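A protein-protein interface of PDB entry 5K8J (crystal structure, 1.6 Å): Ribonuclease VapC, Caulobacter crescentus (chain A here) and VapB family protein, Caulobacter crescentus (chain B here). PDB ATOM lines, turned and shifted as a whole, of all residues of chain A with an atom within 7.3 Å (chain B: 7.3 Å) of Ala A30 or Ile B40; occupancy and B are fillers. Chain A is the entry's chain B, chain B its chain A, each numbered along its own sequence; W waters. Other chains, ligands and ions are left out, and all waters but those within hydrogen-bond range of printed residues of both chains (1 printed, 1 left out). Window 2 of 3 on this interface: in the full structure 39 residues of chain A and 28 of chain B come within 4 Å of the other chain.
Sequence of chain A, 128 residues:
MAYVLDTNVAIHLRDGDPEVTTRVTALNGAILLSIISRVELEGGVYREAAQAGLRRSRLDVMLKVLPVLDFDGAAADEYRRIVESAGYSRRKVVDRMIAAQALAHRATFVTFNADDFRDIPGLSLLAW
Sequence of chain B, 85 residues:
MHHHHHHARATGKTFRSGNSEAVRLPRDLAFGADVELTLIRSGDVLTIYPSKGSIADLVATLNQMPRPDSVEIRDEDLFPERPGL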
ATOM      1  N   ALA A   2     -15.933 -19.624  -0.338  1.00  0.00           N
ATOM      2  CA  ALA A   2     -15.654 -18.992  -1.632  1.00  0.00           C
ATOM      3  C   ALA A   2     -15.932 -19.930  -2.804  1.00  0.00           C
ATOM      4  O   ALA A   2     -15.930 -21.146  -2.652  1.00  0.00           O
ATOM      5  CB  ALA A   2     -14.223 -18.511  -1.691  1.00  0.00           C
ATOM      6  N   TYR A   3     -16.162 -19.324  -3.970  1.00  0.00           N
ATOM      7  CA  TYR A   3     -16.521 -20.030  -5.196  1.00  0.00           C
ATOM      8  C   TYR A   3     -15.597 -19.567  -6.306  1.00  0.00           C
ATOM      9  O   TYR A   3     -15.311 -18.374  -6.421  1.00  0.00           O
ATOM     10  CB  TYR A   3     -17.982 -19.751  -5.604  1.00  0.00           C
ATOM     11  CG  TYR A   3     -18.950 -20.188  -4.533  1.00  0.00           C
ATOM     12  CD1 TYR A   3     -19.400 -21.490  -4.483  1.00  0.00           C
ATOM     13  CD2 TYR A   3     -19.370 -19.303  -3.555  1.00  0.00           C
ATOM     14  CE1 TYR A   3     -20.261 -21.900  -3.497  1.00  0.00           C
ATOM     15  CE2 TYR A   3     -20.236 -19.703  -2.558  1.00  0.00           C
ATOM     16  CZ  TYR A   3     -20.682 -21.005  -2.538  1.00  0.00           C
ATOM     17  OH  TYR A   3     -21.530 -21.452  -1.543  1.00  0.00           O
ATOM     18  N   VAL A   4     -15.134 -20.513  -7.113  1.00  0.00           N
ATOM     19  CA  VAL A   4     -14.478 -20.213  -8.391  1.00  0.00           C
ATOM     20  C   VAL A   4     -15.457 -20.529  -9.510  1.00  0.00           C
ATOM     21  O   VAL A   4     -15.966 -21.654  -9.589  1.00  0.00           O
ATOM     22  CB  VAL A   4     -13.196 -21.036  -8.557  1.00  0.00           C
ATOM     23  CG1 VAL A   4     -12.590 -20.821  -9.949  1.00  0.00           C
ATOM     24  CG2 VAL A   4     -12.178 -20.657  -7.504  1.00  0.00           C
ATOM     25  N   LEU A   5     -15.728 -19.554 -10.387  1.00  0.00           N
ATOM     26  CA  LEU A   5     -16.638 -19.764 -11.499  1.00  0.00           C
ATOM     27  C   LEU A   5     -15.885 -20.403 -12.648  1.00  0.00           C
ATOM     28  O   LEU A   5     -14.834 -19.900 -13.055  1.00  0.00           O
ATOM     29  CB  LEU A   5     -17.233 -18.436 -11.983  1.00  0.00           C
ATOM     30  CG  LEU A   5     -18.021 -17.640 -10.949  1.00  0.00           C
ATOM     31  CD1 LEU A   5     -18.736 -16.409 -11.612  1.00  0.00           C
ATOM     32  CD2 LEU A   5     -19.066 -18.504 -10.259  1.00  0.00           C
ATOM     33  N   LEU A  27     -25.154 -17.203  -4.514  1.00  0.00           N
ATOM     34  CA  LEU A  27     -23.968 -17.781  -3.891  1.00  0.00           C
ATOM     35  C   LEU A  27     -23.642 -17.030  -2.601  1.00  0.00           C
ATOM     36  O   LEU A  27     -23.599 -15.797  -2.574  1.00  0.00           O
ATOM     37  CB  LEU A  27     -22.791 -17.734  -4.866  1.00  0.00           C
ATOM     38  CG  LEU A  27     -22.927 -18.619  -6.115  1.00  0.00           C
ATOM     39  CD1 LEU A  27     -21.816 -18.401  -7.105  1.00  0.00           C
ATOM     40  CD2 LEU A  27     -22.963 -20.098  -5.715  1.00  0.00           C
ATOM     41  N   ASN A  28     -23.443 -17.774  -1.518  1.00  0.00           N
ATOM     42  CA  ASN A  28     -23.152 -17.174  -0.217  1.00  0.00           C
ATOM     43  C   ASN A  28     -21.660 -17.318   0.054  1.00  0.00           C
ATOM     44  O   ASN A  28     -21.201 -18.213   0.774  1.00  0.00           O
ATOM     45  CB  ASN A  28     -23.984 -17.823   0.883  1.00  0.00           C
ATOM     46  CG  ASN A  28     -23.853 -17.093   2.218  1.00  0.00           C
ATOM     47  OD1 ASN A  28     -23.289 -15.997   2.286  1.00  0.00           O
ATOM     48  ND2 ASN A  28     -24.389 -17.690   3.281  1.00  0.00           N
ATOM     49  N   GLY A  29     -20.891 -16.431  -0.562  1.00  0.00           N
ATOM     50  CA  GLY A  29     -19.462 -16.403  -0.342  1.00  0.00           C
ATOM     51  C   GLY A  29     -18.777 -15.556  -1.393  1.00  0.00           C
ATOM     52  O   GLY A  29     -19.401 -15.007  -2.303  1.00  0.00           O
ATOM     53  N   ALA A  30     -17.463 -15.462  -1.241  1.00  0.00           N
ATOM     54  CA  ALA A  30     -16.654 -14.730  -2.205  1.00  0.00           C
ATOM     55  C   ALA A  30     -16.736 -15.410  -3.564  1.00  0.00           C
ATOM     56  O   ALA A  30     -16.692 -16.642  -3.662  1.00  0.00           O
ATOM     57  CB  ALA A  30     -15.196 -14.683  -1.751  1.00  0.00           C
ATOM     58  N   ILE A  31     -16.788 -14.607  -4.613  1.00  0.00           N
ATOM     59  CA  ILE A  31     -16.822 -15.106  -5.984  1.00  0.00           C
ATOM     60  C   ILE A  31     -15.514 -14.740  -6.667  1.00  0.00           C
ATOM     61  O   ILE A  31     -15.170 -13.555  -6.773  1.00  0.00           O
ATOM     62  CB  ILE A  31     -18.043 -14.541  -6.721  1.00  0.00           C
ATOM     63  CG1 ILE A  31     -19.301 -15.091  -6.023  1.00  0.00           C
ATOM     64  CG2 ILE A  31     -17.996 -14.936  -8.184  1.00  0.00           C
ATOM     65  CD1 ILE A  31     -20.582 -14.583  -6.575  1.00  0.00           C
ATOM     66  N   LEU A  32     -14.788 -15.753  -7.122  1.00  0.00           N
ATOM     67  CA  LEU A  32     -13.426 -15.603  -7.617  1.00  0.00           C
ATOM     68  C   LEU A  32     -13.379 -15.994  -9.081  1.00  0.00           C
ATOM     69  O   LEU A  32     -14.073 -16.910  -9.508  1.00  0.00           O
ATOM     70  CB  LEU A  32     -12.452 -16.488  -6.831  1.00  0.00           C
ATOM     71  CG  LEU A  32     -12.576 -16.476  -5.310  1.00  0.00           C
ATOM     72  CD1 LEU A  32     -11.542 -17.420  -4.693  1.00  0.00           C
ATOM     73  CD2 LEU A  32     -12.409 -15.072  -4.742  1.00  0.00           C
ATOM     74  N   PRO A  67     -12.479 -10.349  -7.996  1.00  0.00           N
ATOM     75  CA  PRO A  67     -11.067 -10.602  -7.748  1.00  0.00           C
ATOM     76  C   PRO A  67     -10.566 -11.771  -8.583  1.00  0.00           C
ATOM     77  O   PRO A  67     -11.275 -12.759  -8.785  1.00  0.00           O
ATOM     78  CB  PRO A  67     -11.041 -10.927  -6.252  1.00  0.00           C
ATOM     79  CG  PRO A  67     -12.336 -11.572  -6.026  1.00  0.00           C
ATOM     80  CD  PRO A  67     -13.324 -10.831  -6.892  1.00  0.00           C
ATOM     81  N   ALA A 107     -11.780 -23.463  -2.315  1.00  0.00           N
ATOM     82  CA  ALA A 107     -12.992 -22.863  -2.858  1.00  0.00           C
ATOM     83  C   ALA A 107     -13.812 -23.912  -3.596  1.00  0.00           C
ATOM     84  O   ALA A 107     -13.261 -24.867  -4.154  1.00  0.00           O
ATOM     85  CB  ALA A 107     -12.643 -21.727  -3.820  1.00  0.00           C
ATOM     86  N   THR A 108     -15.129 -23.715  -3.614  1.00  0.00           N
ATOM     87  CA  THR A 108     -16.021 -24.581  -4.373  1.00  0.00           C
ATOM     88  C   THR A 108     -16.055 -24.152  -5.831  1.00  0.00           C
ATOM     89  O   THR A 108     -16.101 -22.958  -6.143  1.00  0.00           O
ATOM     90  CB  THR A 108     -17.402 -24.538  -3.741  1.00  0.00           C
ATOM     91  OG1 THR A 108     -17.323 -25.106  -2.424  1.00  0.00           O
ATOM     92  CG2 THR A 108     -18.453 -25.308  -4.554  1.00  0.00           C
ATOM     93  N   THR B  38     -12.210  -6.602   1.468  1.00  0.00           N
ATOM     94  CA  THR B  38     -13.340  -7.420   1.856  1.00  0.00           C
ATOM     95  C   THR B  38     -12.803  -8.720   2.464  1.00  0.00           C
ATOM     96  O   THR B  38     -11.895  -9.345   1.907  1.00  0.00           O
ATOM     97  CB  THR B  38     -14.221  -7.706   0.638  1.00  0.00           C
ATOM     98  OG1 THR B  38     -14.879  -6.491   0.239  1.00  0.00           O
ATOM     99  CG2 THR B  38     -15.260  -8.737   0.971  1.00  0.00           C
ATOM    100  N   LEU B  39     -13.355  -9.101   3.606  1.00  0.00           N
ATOM    101  CA  LEU B  39     -12.963 -10.290   4.355  1.00  0.00           C
ATOM    102  C   LEU B  39     -14.202 -11.154   4.516  1.00  0.00           C
ATOM    103  O   LEU B  39     -15.188 -10.720   5.114  1.00  0.00           O
ATOM    104  CB  LEU B  39     -12.407  -9.922   5.731  1.00  0.00           C
ATOM    105  CG  LEU B  39     -11.153  -9.044   5.746  1.00  0.00           C
ATOM    106  CD1 LEU B  39     -11.518  -7.581   5.692  1.00  0.00           C
ATOM    107  CD2 LEU B  39     -10.363  -9.345   7.019  1.00  0.00           C
ATOM    108  N   ILE B  40     -14.150 -12.377   4.004  1.00  0.00           N
ATOM    109  CA  ILE B  40     -15.306 -13.259   4.067  1.00  0.00           C
ATOM    110  C   ILE B  40     -14.879 -14.618   4.585  1.00  0.00           C
ATOM    111  O   ILE B  40     -13.963 -15.240   4.027  1.00  0.00           O
ATOM    112  CB  ILE B  40     -15.985 -13.419   2.693  1.00  0.00           C
ATOM    113  CG1 ILE B  40     -16.324 -12.057   2.100  1.00  0.00           C
ATOM    114  CG2 ILE B  40     -17.264 -14.243   2.856  1.00  0.00           C
ATOM    115  CD1 ILE B  40     -16.917 -12.128   0.684  1.00  0.00           C
ATOM    116  N   ARG B  41     -15.568 -15.084   5.620  1.00  0.00           N
ATOM    117  CA  ARG B  41     -15.312 -16.400   6.190  1.00  0.00           C
ATOM    118  C   ARG B  41     -16.403 -17.385   5.792  1.00  0.00           C
ATOM    119  O   ARG B  41     -17.594 -17.079   5.883  1.00  0.00           O
ATOM    120  CB  ARG B  41     -15.226 -16.328   7.702  1.00  0.00           C
ATOM    121  CG  ARG B  41     -14.930 -17.706   8.326  1.00  0.00           C
ATOM    122  CD  ARG B  41     -14.883 -17.632   9.846  1.00  0.00           C
ATOM    123  NE  ARG B  41     -16.120 -17.102  10.423  1.00  0.00           N
ATOM    124  CZ  ARG B  41     -17.226 -17.814  10.654  1.00  0.00           C
ATOM    125  NH1 ARG B  41     -17.281 -19.104  10.362  1.00  0.00           N
ATOM    126  NH2 ARG B  41     -18.291 -17.226  11.177  1.00  0.00           N
ATOM    127  N   SER B  42     -15.992 -18.574   5.373  1.00  0.00           N
ATOM    128  CA  SER B  42     -16.925 -19.679   5.188  1.00  0.00           C
ATOM    129  C   SER B  42     -16.325 -20.855   5.929  1.00  0.00           C
ATOM    130  O   SER B  42     -15.272 -21.352   5.527  1.00  0.00           O
ATOM    131  CB  SER B  42     -17.124 -19.996   3.707  1.00  0.00           C
ATOM    132  OG  SER B  42     -17.914 -21.164   3.538  1.00  0.00           O
ATOM    133  N   VAL B  45     -12.371 -21.128   6.518  1.00  0.00           N
ATOM    134  CA  VAL B  45     -11.609 -20.532   5.430  1.00  0.00           C
ATOM    135  C   VAL B  45     -11.957 -19.052   5.329  1.00  0.00           C
ATOM    136  O   VAL B  45     -13.126 -18.680   5.154  1.00  0.00           O
ATOM    137  CB  VAL B  45     -11.874 -21.240   4.098  1.00  0.00           C
ATOM    138  CG1 VAL B  45     -11.046 -20.638   2.990  1.00  0.00           C
ATOM    139  CG2 VAL B  45     -11.557 -22.723   4.231  1.00  0.00           C
ATOM    140  N   LEU B  46     -10.931 -18.214   5.403  1.00  0.00           N
ATOM    141  CA  LEU B  46     -11.084 -16.775   5.285  1.00  0.00           C
ATOM    142  C   LEU B  46     -10.530 -16.328   3.946  1.00  0.00           C
ATOM    143  O   LEU B  46      -9.404 -16.684   3.587  1.00  0.00           O
ATOM    144  CB  LEU B  46     -10.336 -16.090   6.427  1.00  0.00           C
ATOM    145  CG  LEU B  46     -10.356 -14.572   6.470  1.00  0.00           C
ATOM    146  CD1 LEU B  46     -11.761 -14.082   6.735  1.00  0.00           C
ATOM    147  CD2 LEU B  46      -9.394 -14.128   7.588  1.00  0.00           C
ATOM    148  N   THR B  47     -11.328 -15.563   3.186  1.00  0.00           N
ATOM    149  CA  THR B  47     -10.939 -15.082   1.867  1.00  0.00           C
ATOM    150  C   THR B  47     -10.922 -13.558   1.900  1.00  0.00           C
ATOM    151  O   THR B  47     -11.899 -12.940   2.339  1.00  0.00           O
ATOM    152  CB  THR B  47     -11.915 -15.584   0.799  1.00  0.00           C
ATOM    153  OG1 THR B  47     -11.930 -17.009   0.786  1.00  0.00           O
ATOM    154  CG2 THR B  47     -11.509 -15.102  -0.582  1.00  0.00           C
ATOM    155  N   ILE B  48      -9.821 -12.969   1.444  1.00  0.00           N
ATOM    156  CA  ILE B  48      -9.572 -11.531   1.570  1.00  0.00           C
ATOM    157  C   ILE B  48      -9.167 -10.992   0.201  1.00  0.00           C
ATOM    158  O   ILE B  48      -8.336 -11.597  -0.482  1.00  0.00           O
ATOM    159  CB  ILE B  48      -8.465 -11.272   2.616  1.00  0.00           C
ATOM    160  CG1 ILE B  48      -8.874 -11.856   3.968  1.00  0.00           C
ATOM    161  CG2 ILE B  48      -8.187  -9.779   2.752  1.00  0.00           C
ATOM    162  CD1 ILE B  48      -7.806 -11.718   5.058  1.00  0.00           C
ATOM    163  N   TYR B  49      -9.803  -9.903  -0.242  1.00  0.00           N
ATOM    164  CA  TYR B  49      -9.508  -9.357  -1.563  1.00  0.00           C
ATOM    165  C   TYR B  49      -9.902  -7.884  -1.570  1.00  0.00           C
ATOM    166  O   TYR B  49     -10.613  -7.417  -0.672  1.00  0.00           O
ATOM    167  CB  TYR B  49     -10.236 -10.133  -2.679  1.00  0.00           C
ATOM    168  CG  TYR B  49     -11.720 -10.194  -2.551  1.00  0.00           C
ATOM    169  CD1 TYR B  49     -12.519  -9.194  -3.112  1.00  0.00           C
ATOM    170  CD2 TYR B  49     -12.341 -11.215  -1.862  1.00  0.00           C
ATOM    171  CE1 TYR B  49     -13.897  -9.211  -2.977  1.00  0.00           C
ATOM    172  CE2 TYR B  49     -13.733 -11.244  -1.723  1.00  0.00           C
ATOM    173  CZ  TYR B  49     -14.495 -10.245  -2.299  1.00  0.00           C
ATOM    174  OH  TYR B  49     -15.865 -10.249  -2.178  1.00  0.00           O
ATOM    175  N   ILE B  55     -21.374  -7.914  -5.474  1.00  0.00           N
ATOM    176  CA  ILE B  55     -21.920  -8.728  -6.556  1.00  0.00           C
ATOM    177  C   ILE B  55     -23.274  -8.200  -6.990  1.00  0.00           C
ATOM    178  O   ILE B  55     -23.576  -8.148  -8.189  1.00  0.00           O
ATOM    179  CB  ILE B  55     -21.993 -10.200  -6.133  1.00  0.00           C
ATOM    180  CG1 ILE B  55     -20.592 -10.697  -5.800  1.00  0.00           C
ATOM    181  CG2 ILE B  55     -22.607 -11.071  -7.228  1.00  0.00           C
ATOM    182  CD1 ILE B  55     -19.595 -10.566  -6.943  1.00  0.00           C
HETATM  183  O   HOH W   1     -18.460 -20.592   0.477  1.00  0.00           O
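N of Thr B38 lies within hydrogen-bond range of O of Tyr B49 (2.8 Å). The backbone carbonyl oxygen (O) of Ile B40 sits at hydrogen-bond distance from the backbone NH (N) of Thr B47 (2.8 Å). The backbone carbonyl oxygen (O) of Ala A30 lies within hydrogen-bond range of the backbone NH (N) of Tyr A3, 2.8 Å away. The backbone NH (N) of Thr A108 lies within hydrogen-bond range of the backbone carbonyl oxygen (O) of Ala A2, 2.9 Å away.
Thr B47 touches Ala A2 (OG1 to CB, 3.7 Å). Ala A30 touches Ile B40. Ala A30 touches Thr B47 (CB to CG2, 3.9 Å). Ala A30 touches Tyr B49. CD1 of Ile A31 touches CG1 of Ile B55 (3.96 Å). Tyr B49 touches Pro A67 (CB to CB, 3.7 Å).
Asn A28 touches none of the printed residues of chain B. Ala A30 touches three residues of chain B. Of the printed residues of chain B, Ile A31 touches Ile B55 (3.96 Å). Ile B40 touches just one residue of chain A: Ala A30. Printed residues of chain A within 4 Å of Thr B47: Ala A2 and Ala A30. Of the printed residues of chain A, Tyr B49 touches Ala A30 (3.7 Å) and Pro A67 (3.7 Å). The nearest residue of chain A that does not touch Ile B40 is Gly A29 (4.4 Å).
Hydrophobic or aromatic side chains of chain B within 4 Å of the printed part of chain A: Ile B40, Tyr B49 and Ile B55. Along chain B the printed residues that touch a printed residue of chain A span positions 40 to 55. Of the 13 printed residues of chain A, 4 touch a printed residue of chain B. Printed residues of chain A that touch a printed residue of chain B: Ala A2, Ala A30, Ile A31 and Pro A67. Hydrophobic or aromatic side chains of chain A that line the printed part of chain B: Ala A2, Ala A30, Ile A31 and Pro A67. Along chain A the printed residues that touch a printed residue of chain B span positions 2 to 67.
Water W1 bridges the backbone NH (N) of Ala A2 (2.8 Å) and the side-chain hydroxyl (OG) of Ser B42 (3.2 Å).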
